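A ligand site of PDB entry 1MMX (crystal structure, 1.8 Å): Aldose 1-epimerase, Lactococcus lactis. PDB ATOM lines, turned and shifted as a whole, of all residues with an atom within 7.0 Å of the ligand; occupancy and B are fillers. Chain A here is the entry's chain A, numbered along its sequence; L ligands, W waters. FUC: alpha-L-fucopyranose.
O3 of the ligand is in hydrogen-bond range of OD2 of Asp 243, 2.5 Å away. An oxygen (O1) of the ligand sits at hydrogen-bond distance from the side-chain carboxylate (OE2) of Glu 304 (2.7 Å). A ring nitrogen (NE2) of His 170 sits at hydrogen-bond distance from an oxygen (O5) of the ligand, at 2.8 Å. An oxygen (O5) of the ligand lies within hydrogen-bond range of a ring nitrogen (NE2) of His 96 (3.0 Å). The guanidinium group (NH1) of Arg 71 lies within hydrogen-bond range of an oxygen (O3) of the ligand (3.0 Å). An oxygen (O3) of the ligand is in hydrogen-bond range of the side-chain carboxylate (OE2) of Glu 203 (3.3 Å).
OD2 of Asp 243 sits close to OE2 of Glu 203. The backbone NH (N) of Asp 243 sits close to the backbone carbonyl oxygen (O) of Ile 278, at 3.4 Å. The side-chain carboxylate (OE2) of Glu 304 is in hydrogen-bond range of the side-chain hydroxyl (OG1) of Thr 302 (2.8 Å). The backbone NH (N) of His 96 sits at hydrogen-bond distance from the backbone carbonyl oxygen (O) of Gly 70 (2.9 Å). The side-chain carboxylate (OE2) of Glu 203 is in salt-bridge range of the guanidinium group (NH1) of Arg 71, at 3.7 Å. The side-chain carboxylate (OE1) of Glu 90 is in salt-bridge range of the guanidinium group (NE) of Arg 71, at 2.9 Å. The backbone carbonyl oxygen of Phe 279 is in hydrogen-bond range of the backbone NH of Thr 302, 3.0 Å away. N of Tyr 60 lies within hydrogen-bond range of OD1 of Asp 58 (3.0 Å).
Tyr 60 touches the ligand (CD1 to C6, 3.9 Å). OH of Tyr 172 touches C6 of the ligand (3.9 Å). CB of Phe 279 touches O1 of the ligand, 3.2 Å away. Within 4 Å of the ligand: Tyr 60, Arg 71, His 96, His 170, Tyr 172, Glu 203, Asp 243, Phe 279 and Glu 304.
Water W1 lies within hydrogen-bond range of an oxygen (O3) of the ligand (2.6 Å), the side-chain carboxylate (OE2) of Glu 203 (3.4 Å) and the side-chain carboxylate (OD2) of Asp 243 (3.5 Å). Water W3 lies within hydrogen-bond range of OH of Tyr 172 and OD2 of Asp 58.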
ATOM      1  N   ASP A  58      -0.391 -13.945 -26.398  1.00  0.00           N
ATOM      2  CA  ASP A  58      -0.615 -15.331 -26.067  1.00  0.00           C
ATOM      3  C   ASP A  58      -2.061 -15.545 -26.373  1.00  0.00           C
ATOM      4  O   ASP A  58      -2.885 -14.831 -25.801  1.00  0.00           O
ATOM      5  CB  ASP A  58      -0.276 -15.665 -24.595  1.00  0.00           C
ATOM      6  CG  ASP A  58      -0.552 -17.116 -24.259  1.00  0.00           C
ATOM      7  OD1 ASP A  58      -0.996 -17.934 -25.042  1.00  0.00           O
ATOM      8  OD2 ASP A  58      -0.265 -17.423 -23.027  1.00  0.00           O
ATOM      9  N   TYR A  60      -3.825 -18.370 -25.999  1.00  0.00           N
ATOM     10  CA  TYR A  60      -4.528 -19.408 -25.232  1.00  0.00           C
ATOM     11  C   TYR A  60      -5.418 -18.994 -24.064  1.00  0.00           C
ATOM     12  O   TYR A  60      -6.507 -19.587 -23.826  1.00  0.00           O
ATOM     13  CB  TYR A  60      -3.521 -20.479 -24.758  1.00  0.00           C
ATOM     14  CG  TYR A  60      -3.000 -21.320 -25.919  1.00  0.00           C
ATOM     15  CD1 TYR A  60      -1.633 -21.416 -26.155  1.00  0.00           C
ATOM     16  CD2 TYR A  60      -3.854 -21.988 -26.790  1.00  0.00           C
ATOM     17  CE1 TYR A  60      -1.107 -22.161 -27.204  1.00  0.00           C
ATOM     18  CE2 TYR A  60      -3.367 -22.724 -27.865  1.00  0.00           C
ATOM     19  CZ  TYR A  60      -1.984 -22.818 -28.058  1.00  0.00           C
ATOM     20  OH  TYR A  60      -1.490 -23.560 -29.098  1.00  0.00           O
ATOM     21  N   PRO A  61      -4.997 -17.984 -23.298  1.00  0.00           N
ATOM     22  CA  PRO A  61      -5.775 -17.579 -22.115  1.00  0.00           C
ATOM     23  C   PRO A  61      -7.271 -17.435 -22.325  1.00  0.00           C
ATOM     24  O   PRO A  61      -7.693 -16.633 -23.116  1.00  0.00           O
ATOM     25  CB  PRO A  61      -5.171 -16.254 -21.668  1.00  0.00           C
ATOM     26  CG  PRO A  61      -3.759 -16.258 -22.215  1.00  0.00           C
ATOM     27  CD  PRO A  61      -3.817 -17.118 -23.467  1.00  0.00           C
ATOM     28  N   GLY A  70      -4.552 -30.369 -25.579  1.00  0.00           N
ATOM     29  CA  GLY A  70      -3.386 -31.080 -25.106  1.00  0.00           C
ATOM     30  C   GLY A  70      -2.443 -31.497 -26.196  1.00  0.00           C
ATOM     31  O   GLY A  70      -2.568 -31.103 -27.344  1.00  0.00           O
ATOM     32  N   ARG A  71      -1.466 -32.313 -25.799  1.00  0.00           N
ATOM     33  CA  ARG A  71      -0.476 -32.801 -26.717  1.00  0.00           C
ATOM     34  C   ARG A  71      -0.734 -34.196 -27.209  1.00  0.00           C
ATOM     35  O   ARG A  71      -1.032 -35.095 -26.402  1.00  0.00           O
ATOM     36  CB  ARG A  71       0.869 -32.911 -26.055  1.00  0.00           C
ATOM     37  CG  ARG A  71       1.371 -31.562 -25.673  1.00  0.00           C
ATOM     38  CD  ARG A  71       2.668 -31.588 -24.851  1.00  0.00           C
ATOM     39  NE  ARG A  71       3.092 -30.190 -24.772  1.00  0.00           N
ATOM     40  CZ  ARG A  71       2.716 -29.332 -23.836  1.00  0.00           C
ATOM     41  NH1 ARG A  71       1.976 -29.673 -22.758  1.00  0.00           N
ATOM     42  NH2 ARG A  71       3.165 -28.106 -23.989  1.00  0.00           N
ATOM     43  N   GLU A  90       4.411 -28.149 -32.296  1.00  0.00           N
ATOM     44  CA  GLU A  90       5.280 -28.084 -31.124  1.00  0.00           C
ATOM     45  C   GLU A  90       6.201 -29.240 -31.332  1.00  0.00           C
ATOM     46  O   GLU A  90       5.973 -30.345 -30.827  1.00  0.00           O
ATOM     47  CB  GLU A  90       4.479 -28.315 -29.843  1.00  0.00           C
ATOM     48  CG  GLU A  90       5.301 -27.785 -28.674  1.00  0.00           C
ATOM     49  CD  GLU A  90       4.831 -28.293 -27.338  1.00  0.00           C
ATOM     50  OE1 GLU A  90       4.589 -29.441 -27.109  1.00  0.00           O
ATOM     51  OE2 GLU A  90       4.697 -27.372 -26.417  1.00  0.00           O
ATOM     52  N   LEU A  95      -0.175 -29.788 -30.561  1.00  0.00           N
ATOM     53  CA  LEU A  95      -0.577 -29.197 -29.282  1.00  0.00           C
ATOM     54  C   LEU A  95      -1.814 -28.348 -29.476  1.00  0.00           C
ATOM     55  O   LEU A  95      -1.816 -27.497 -30.341  1.00  0.00           O
ATOM     56  CB  LEU A  95       0.559 -28.271 -28.759  1.00  0.00           C
ATOM     57  CG  LEU A  95       0.078 -27.339 -27.637  1.00  0.00           C
ATOM     58  CD1 LEU A  95      -0.129 -28.114 -26.328  1.00  0.00           C
ATOM     59  CD2 LEU A  95       1.096 -26.233 -27.399  1.00  0.00           C
ATOM     60  N   HIS A  96      -2.838 -28.594 -28.702  1.00  0.00           N
ATOM     61  CA  HIS A  96      -4.083 -27.815 -28.812  1.00  0.00           C
ATOM     62  C   HIS A  96      -4.678 -27.679 -30.221  1.00  0.00           C
ATOM     63  O   HIS A  96      -5.116 -26.595 -30.611  1.00  0.00           O
ATOM     64  CB  HIS A  96      -3.900 -26.414 -28.160  1.00  0.00           C
ATOM     65  CG  HIS A  96      -3.549 -26.494 -26.699  1.00  0.00           C
ATOM     66  ND1 HIS A  96      -4.095 -27.472 -25.881  1.00  0.00           N
ATOM     67  CD2 HIS A  96      -2.748 -25.716 -25.952  1.00  0.00           C
ATOM     68  CE1 HIS A  96      -3.611 -27.287 -24.674  1.00  0.00           C
ATOM     69  NE2 HIS A  96      -2.805 -26.215 -24.672  1.00  0.00           N
ATOM     70  N   HIS A 170      -9.579 -22.848 -21.629  1.00  0.00           N
ATOM     71  CA  HIS A 170      -8.279 -22.595 -21.047  1.00  0.00           C
ATOM     72  C   HIS A 170      -8.119 -21.314 -20.224  1.00  0.00           C
ATOM     73  O   HIS A 170      -7.101 -20.612 -20.334  1.00  0.00           O
ATOM     74  CB  HIS A 170      -7.262 -22.543 -22.185  1.00  0.00           C
ATOM     75  CG  HIS A 170      -5.856 -22.937 -21.836  1.00  0.00           C
ATOM     76  ND1 HIS A 170      -4.971 -22.067 -21.192  1.00  0.00           N
ATOM     77  CD2 HIS A 170      -5.191 -24.083 -22.115  1.00  0.00           C
ATOM     78  CE1 HIS A 170      -3.830 -22.711 -21.053  1.00  0.00           C
ATOM     79  NE2 HIS A 170      -3.927 -23.910 -21.607  1.00  0.00           N
ATOM     80  N   TYR A 172      -7.268 -18.998 -17.045  1.00  0.00           N
ATOM     81  CA  TYR A 172      -6.221 -19.021 -16.019  1.00  0.00           C
ATOM     82  C   TYR A 172      -6.767 -18.176 -14.881  1.00  0.00           C
ATOM     83  O   TYR A 172      -7.180 -17.029 -15.091  1.00  0.00           O
ATOM     84  CB  TYR A 172      -4.968 -18.224 -16.441  1.00  0.00           C
ATOM     85  CG  TYR A 172      -4.018 -18.957 -17.385  1.00  0.00           C
ATOM     86  CD1 TYR A 172      -4.099 -18.761 -18.763  1.00  0.00           C
ATOM     87  CD2 TYR A 172      -3.018 -19.810 -16.906  1.00  0.00           C
ATOM     88  CE1 TYR A 172      -3.227 -19.392 -19.642  1.00  0.00           C
ATOM     89  CE2 TYR A 172      -2.136 -20.460 -17.756  1.00  0.00           C
ATOM     90  CZ  TYR A 172      -2.236 -20.236 -19.135  1.00  0.00           C
ATOM     91  OH  TYR A 172      -1.358 -20.877 -19.988  1.00  0.00           O
ATOM     92  N   LEU A 198       4.613 -37.130 -16.924  1.00  0.00           N
ATOM     93  CA  LEU A 198       5.096 -36.777 -18.226  1.00  0.00           C
ATOM     94  C   LEU A 198       6.426 -37.463 -18.514  1.00  0.00           C
ATOM     95  O   LEU A 198       7.197 -37.756 -17.601  1.00  0.00           O
ATOM     96  CB  LEU A 198       5.214 -35.250 -18.378  1.00  0.00           C
ATOM     97  CG  LEU A 198       3.940 -34.491 -17.969  1.00  0.00           C
ATOM     98  CD1 LEU A 198       4.184 -33.009 -18.232  1.00  0.00           C
ATOM     99  CD2 LEU A 198       2.724 -34.938 -18.784  1.00  0.00           C
ATOM    100  N   GLU A 203       6.933 -33.082 -22.713  1.00  0.00           N
ATOM    101  CA  GLU A 203       5.603 -33.096 -22.148  1.00  0.00           C
ATOM    102  C   GLU A 203       4.658 -34.118 -22.661  1.00  0.00           C
ATOM    103  O   GLU A 203       3.468 -34.039 -22.406  1.00  0.00           O
ATOM    104  CB  GLU A 203       5.000 -31.697 -21.900  1.00  0.00           C
ATOM    105  CG  GLU A 203       5.926 -30.795 -21.031  1.00  0.00           C
ATOM    106  CD  GLU A 203       5.678 -29.286 -20.949  1.00  0.00           C
ATOM    107  OE1 GLU A 203       6.439 -28.433 -21.419  1.00  0.00           O
ATOM    108  OE2 GLU A 203       4.618 -28.967 -20.253  1.00  0.00           O
ATOM    109  N   ASP A 243       1.923 -29.342 -14.416  1.00  0.00           N
ATOM    110  CA  ASP A 243       1.501 -29.308 -15.814  1.00  0.00           C
ATOM    111  C   ASP A 243       1.142 -30.733 -16.098  1.00  0.00           C
ATOM    112  O   ASP A 243       1.836 -31.426 -16.799  1.00  0.00           O
ATOM    113  CB  ASP A 243       2.595 -28.763 -16.760  1.00  0.00           C
ATOM    114  CG  ASP A 243       1.993 -28.415 -18.097  1.00  0.00           C
ATOM    115  OD1 ASP A 243       0.841 -28.572 -18.372  1.00  0.00           O
ATOM    116  OD2 ASP A 243       2.825 -27.851 -18.900  1.00  0.00           O
ATOM    117  N   HIS A 244       0.029 -31.155 -15.465  1.00  0.00           N
ATOM    118  CA  HIS A 244      -0.354 -32.533 -15.508  1.00  0.00           C
ATOM    119  C   HIS A 244      -1.826 -32.789 -15.406  1.00  0.00           C
ATOM    120  O   HIS A 244      -2.569 -32.036 -14.763  1.00  0.00           O
ATOM    121  CB  HIS A 244       0.180 -33.157 -14.162  1.00  0.00           C
ATOM    122  CG  HIS A 244       1.677 -33.240 -14.109  1.00  0.00           C
ATOM    123  ND1 HIS A 244       2.487 -32.142 -13.781  1.00  0.00           N
ATOM    124  CD2 HIS A 244       2.486 -34.282 -14.410  1.00  0.00           C
ATOM    125  CE1 HIS A 244       3.753 -32.549 -13.873  1.00  0.00           C
ATOM    126  NE2 HIS A 244       3.781 -33.827 -14.240  1.00  0.00           N
ATOM    127  N   VAL A 277      -6.596 -31.152 -16.302  1.00  0.00           N
ATOM    128  CA  VAL A 277      -5.204 -30.852 -16.500  1.00  0.00           C
ATOM    129  C   VAL A 277      -4.966 -29.546 -15.741  1.00  0.00           C
ATOM    130  O   VAL A 277      -5.699 -28.573 -15.911  1.00  0.00           O
ATOM    131  CB  VAL A 277      -4.871 -30.667 -17.980  1.00  0.00           C
ATOM    132  CG1 VAL A 277      -3.465 -30.058 -18.115  1.00  0.00           C
ATOM    133  CG2 VAL A 277      -4.925 -32.028 -18.682  1.00  0.00           C
ATOM    134  N   ILE A 278      -3.955 -29.524 -14.876  1.00  0.00           N
ATOM    135  CA  ILE A 278      -3.667 -28.302 -14.114  1.00  0.00           C
ATOM    136  C   ILE A 278      -2.296 -27.794 -14.510  1.00  0.00           C
ATOM    137  O   ILE A 278      -1.336 -28.549 -14.411  1.00  0.00           O
ATOM    138  CB  ILE A 278      -3.666 -28.619 -12.597  1.00  0.00           C
ATOM    139  CG1 ILE A 278      -5.085 -28.981 -12.198  1.00  0.00           C
ATOM    140  CG2 ILE A 278      -3.182 -27.416 -11.761  1.00  0.00           C
ATOM    141  CD1 ILE A 278      -5.234 -29.244 -10.716  1.00  0.00           C
ATOM    142  N   PHE A 279      -2.234 -26.551 -14.976  1.00  0.00           N
ATOM    143  CA  PHE A 279      -0.971 -25.949 -15.402  1.00  0.00           C
ATOM    144  C   PHE A 279      -0.815 -24.646 -14.632  1.00  0.00           C
ATOM    145  O   PHE A 279      -1.709 -23.794 -14.641  1.00  0.00           O
ATOM    146  CB  PHE A 279      -1.078 -25.702 -16.933  1.00  0.00           C
ATOM    147  CG  PHE A 279       0.002 -24.859 -17.496  1.00  0.00           C
ATOM    148  CD1 PHE A 279       1.325 -25.252 -17.365  1.00  0.00           C
ATOM    149  CD2 PHE A 279      -0.319 -23.655 -18.142  1.00  0.00           C
ATOM    150  CE1 PHE A 279       2.360 -24.471 -17.869  1.00  0.00           C
ATOM    151  CE2 PHE A 279       0.713 -22.861 -18.641  1.00  0.00           C
ATOM    152  CZ  PHE A 279       2.033 -23.283 -18.520  1.00  0.00           C
ATOM    153  N   THR A 280       0.298 -24.514 -13.922  1.00  0.00           N
ATOM    154  CA  THR A 280       0.533 -23.332 -13.100  1.00  0.00           C
ATOM    155  C   THR A 280       1.393 -22.229 -13.720  1.00  0.00           C
ATOM    156  O   THR A 280       2.255 -21.648 -13.084  1.00  0.00           O
ATOM    157  CB  THR A 280       1.051 -23.758 -11.708  1.00  0.00           C
ATOM    158  OG1 THR A 280       2.206 -24.558 -11.915  1.00  0.00           O
ATOM    159  CG2 THR A 280      -0.010 -24.642 -11.095  1.00  0.00           C
ATOM    160  N   ASN A 282       3.980 -21.964 -15.605  1.00  0.00           N
ATOM    161  CA  ASN A 282       5.393 -22.099 -15.356  1.00  0.00           C
ATOM    162  C   ASN A 282       6.241 -21.393 -16.405  1.00  0.00           C
ATOM    163  O   ASN A 282       7.110 -22.008 -17.030  1.00  0.00           O
ATOM    164  CB  ASN A 282       5.711 -23.614 -15.327  1.00  0.00           C
ATOM    165  CG  ASN A 282       4.735 -24.377 -14.428  1.00  0.00           C
ATOM    166  OD1 ASN A 282       4.314 -23.865 -13.398  1.00  0.00           O
ATOM    167  ND2 ASN A 282       4.360 -25.593 -14.801  1.00  0.00           N
ATOM    168  N   PHE A 283       6.002 -20.108 -16.640  1.00  0.00           N
ATOM    169  CA  PHE A 283       6.729 -19.389 -17.685  1.00  0.00           C
ATOM    170  C   PHE A 283       8.095 -18.792 -17.357  1.00  0.00           C
ATOM    171  O   PHE A 283       8.694 -18.067 -18.165  1.00  0.00           O
ATOM    172  CB  PHE A 283       5.863 -18.289 -18.300  1.00  0.00           C
ATOM    173  CG  PHE A 283       4.520 -18.795 -18.786  1.00  0.00           C
ATOM    174  CD1 PHE A 283       3.334 -18.340 -18.225  1.00  0.00           C
ATOM    175  CD2 PHE A 283       4.463 -19.679 -19.854  1.00  0.00           C
ATOM    176  CE1 PHE A 283       2.104 -18.771 -18.720  1.00  0.00           C
ATOM    177  CE2 PHE A 283       3.243 -20.145 -20.357  1.00  0.00           C
ATOM    178  CZ  PHE A 283       2.063 -19.670 -19.782  1.00  0.00           C
ATOM    179  N   THR A 302      -4.637 -23.126 -14.364  1.00  0.00           N
ATOM    180  CA  THR A 302      -5.796 -23.547 -15.168  1.00  0.00           C
ATOM    181  C   THR A 302      -6.477 -24.752 -14.569  1.00  0.00           C
ATOM    182  O   THR A 302      -5.941 -25.429 -13.722  1.00  0.00           O
ATOM    183  CB  THR A 302      -5.343 -23.964 -16.597  1.00  0.00           C
ATOM    184  OG1 THR A 302      -4.554 -25.140 -16.493  1.00  0.00           O
ATOM    185  CG2 THR A 302      -4.479 -22.913 -17.315  1.00  0.00           C
ATOM    186  N   GLU A 304      -8.222 -27.323 -16.816  1.00  0.00           N
ATOM    187  CA  GLU A 304      -8.633 -27.777 -18.124  1.00  0.00           C
ATOM    188  C   GLU A 304      -9.326 -29.111 -18.003  1.00  0.00           C
ATOM    189  O   GLU A 304      -8.694 -30.148 -17.948  1.00  0.00           O
ATOM    190  CB  GLU A 304      -7.378 -27.888 -18.996  1.00  0.00           C
ATOM    191  CG  GLU A 304      -6.717 -26.501 -19.151  1.00  0.00           C
ATOM    192  CD  GLU A 304      -5.374 -26.540 -19.825  1.00  0.00           C
ATOM    193  OE1 GLU A 304      -5.191 -27.032 -20.918  1.00  0.00           O
ATOM    194  OE2 GLU A 304      -4.413 -26.008 -19.123  1.00  0.00           O
ATOM    195  N   PRO A 309      -4.976 -36.071 -21.760  1.00  0.00           N
ATOM    196  CA  PRO A 309      -4.169 -36.269 -22.944  1.00  0.00           C
ATOM    197  C   PRO A 309      -3.390 -37.581 -22.771  1.00  0.00           C
ATOM    198  O   PRO A 309      -3.254 -38.053 -21.655  1.00  0.00           O
ATOM    199  CB  PRO A 309      -3.127 -35.116 -22.965  1.00  0.00           C
ATOM    200  CG  PRO A 309      -3.514 -34.150 -21.847  1.00  0.00           C
ATOM    201  CD  PRO A 309      -4.668 -34.783 -21.080  1.00  0.00           C
HETATM  202  C1  FUC L   1      -1.604 -26.461 -21.321  1.00  0.00           C
HETATM  203  C2  FUC L   1      -0.315 -27.251 -21.466  1.00  0.00           C
HETATM  204  C3  FUC L   1       0.818 -26.373 -20.999  1.00  0.00           C
HETATM  205  C4  FUC L   1       0.902 -25.201 -21.946  1.00  0.00           C
HETATM  206  C5  FUC L   1      -0.415 -24.422 -21.883  1.00  0.00           C
HETATM  207  C6  FUC L   1      -0.532 -23.324 -22.930  1.00  0.00           C
HETATM  208  O1  FUC L   1      -1.856 -26.102 -19.963  1.00  0.00           O
HETATM  209  O2  FUC L   1      -0.263 -28.460 -20.698  1.00  0.00           O
HETATM  210  O3  FUC L   1       2.021 -27.114 -21.112  1.00  0.00           O
HETATM  211  O4  FUC L   1       1.166 -25.673 -23.255  1.00  0.00           O
HETATM  212  O5  FUC L   1      -1.548 -25.276 -22.132  1.00  0.00           O
HETATM  213  O   HOH W   1       4.191 -25.771 -21.350  1.00  0.00           O
HETATM  214  O   HOH W   2      -2.160 -30.429 -21.757  1.00  0.00           O
HETATM  215  O   HOH W   3      -0.971 -19.900 -22.384  1.00  0.00           O
HETATM  216  O   HOH W   4       2.237 -23.638 -24.229  1.00  0.00           O
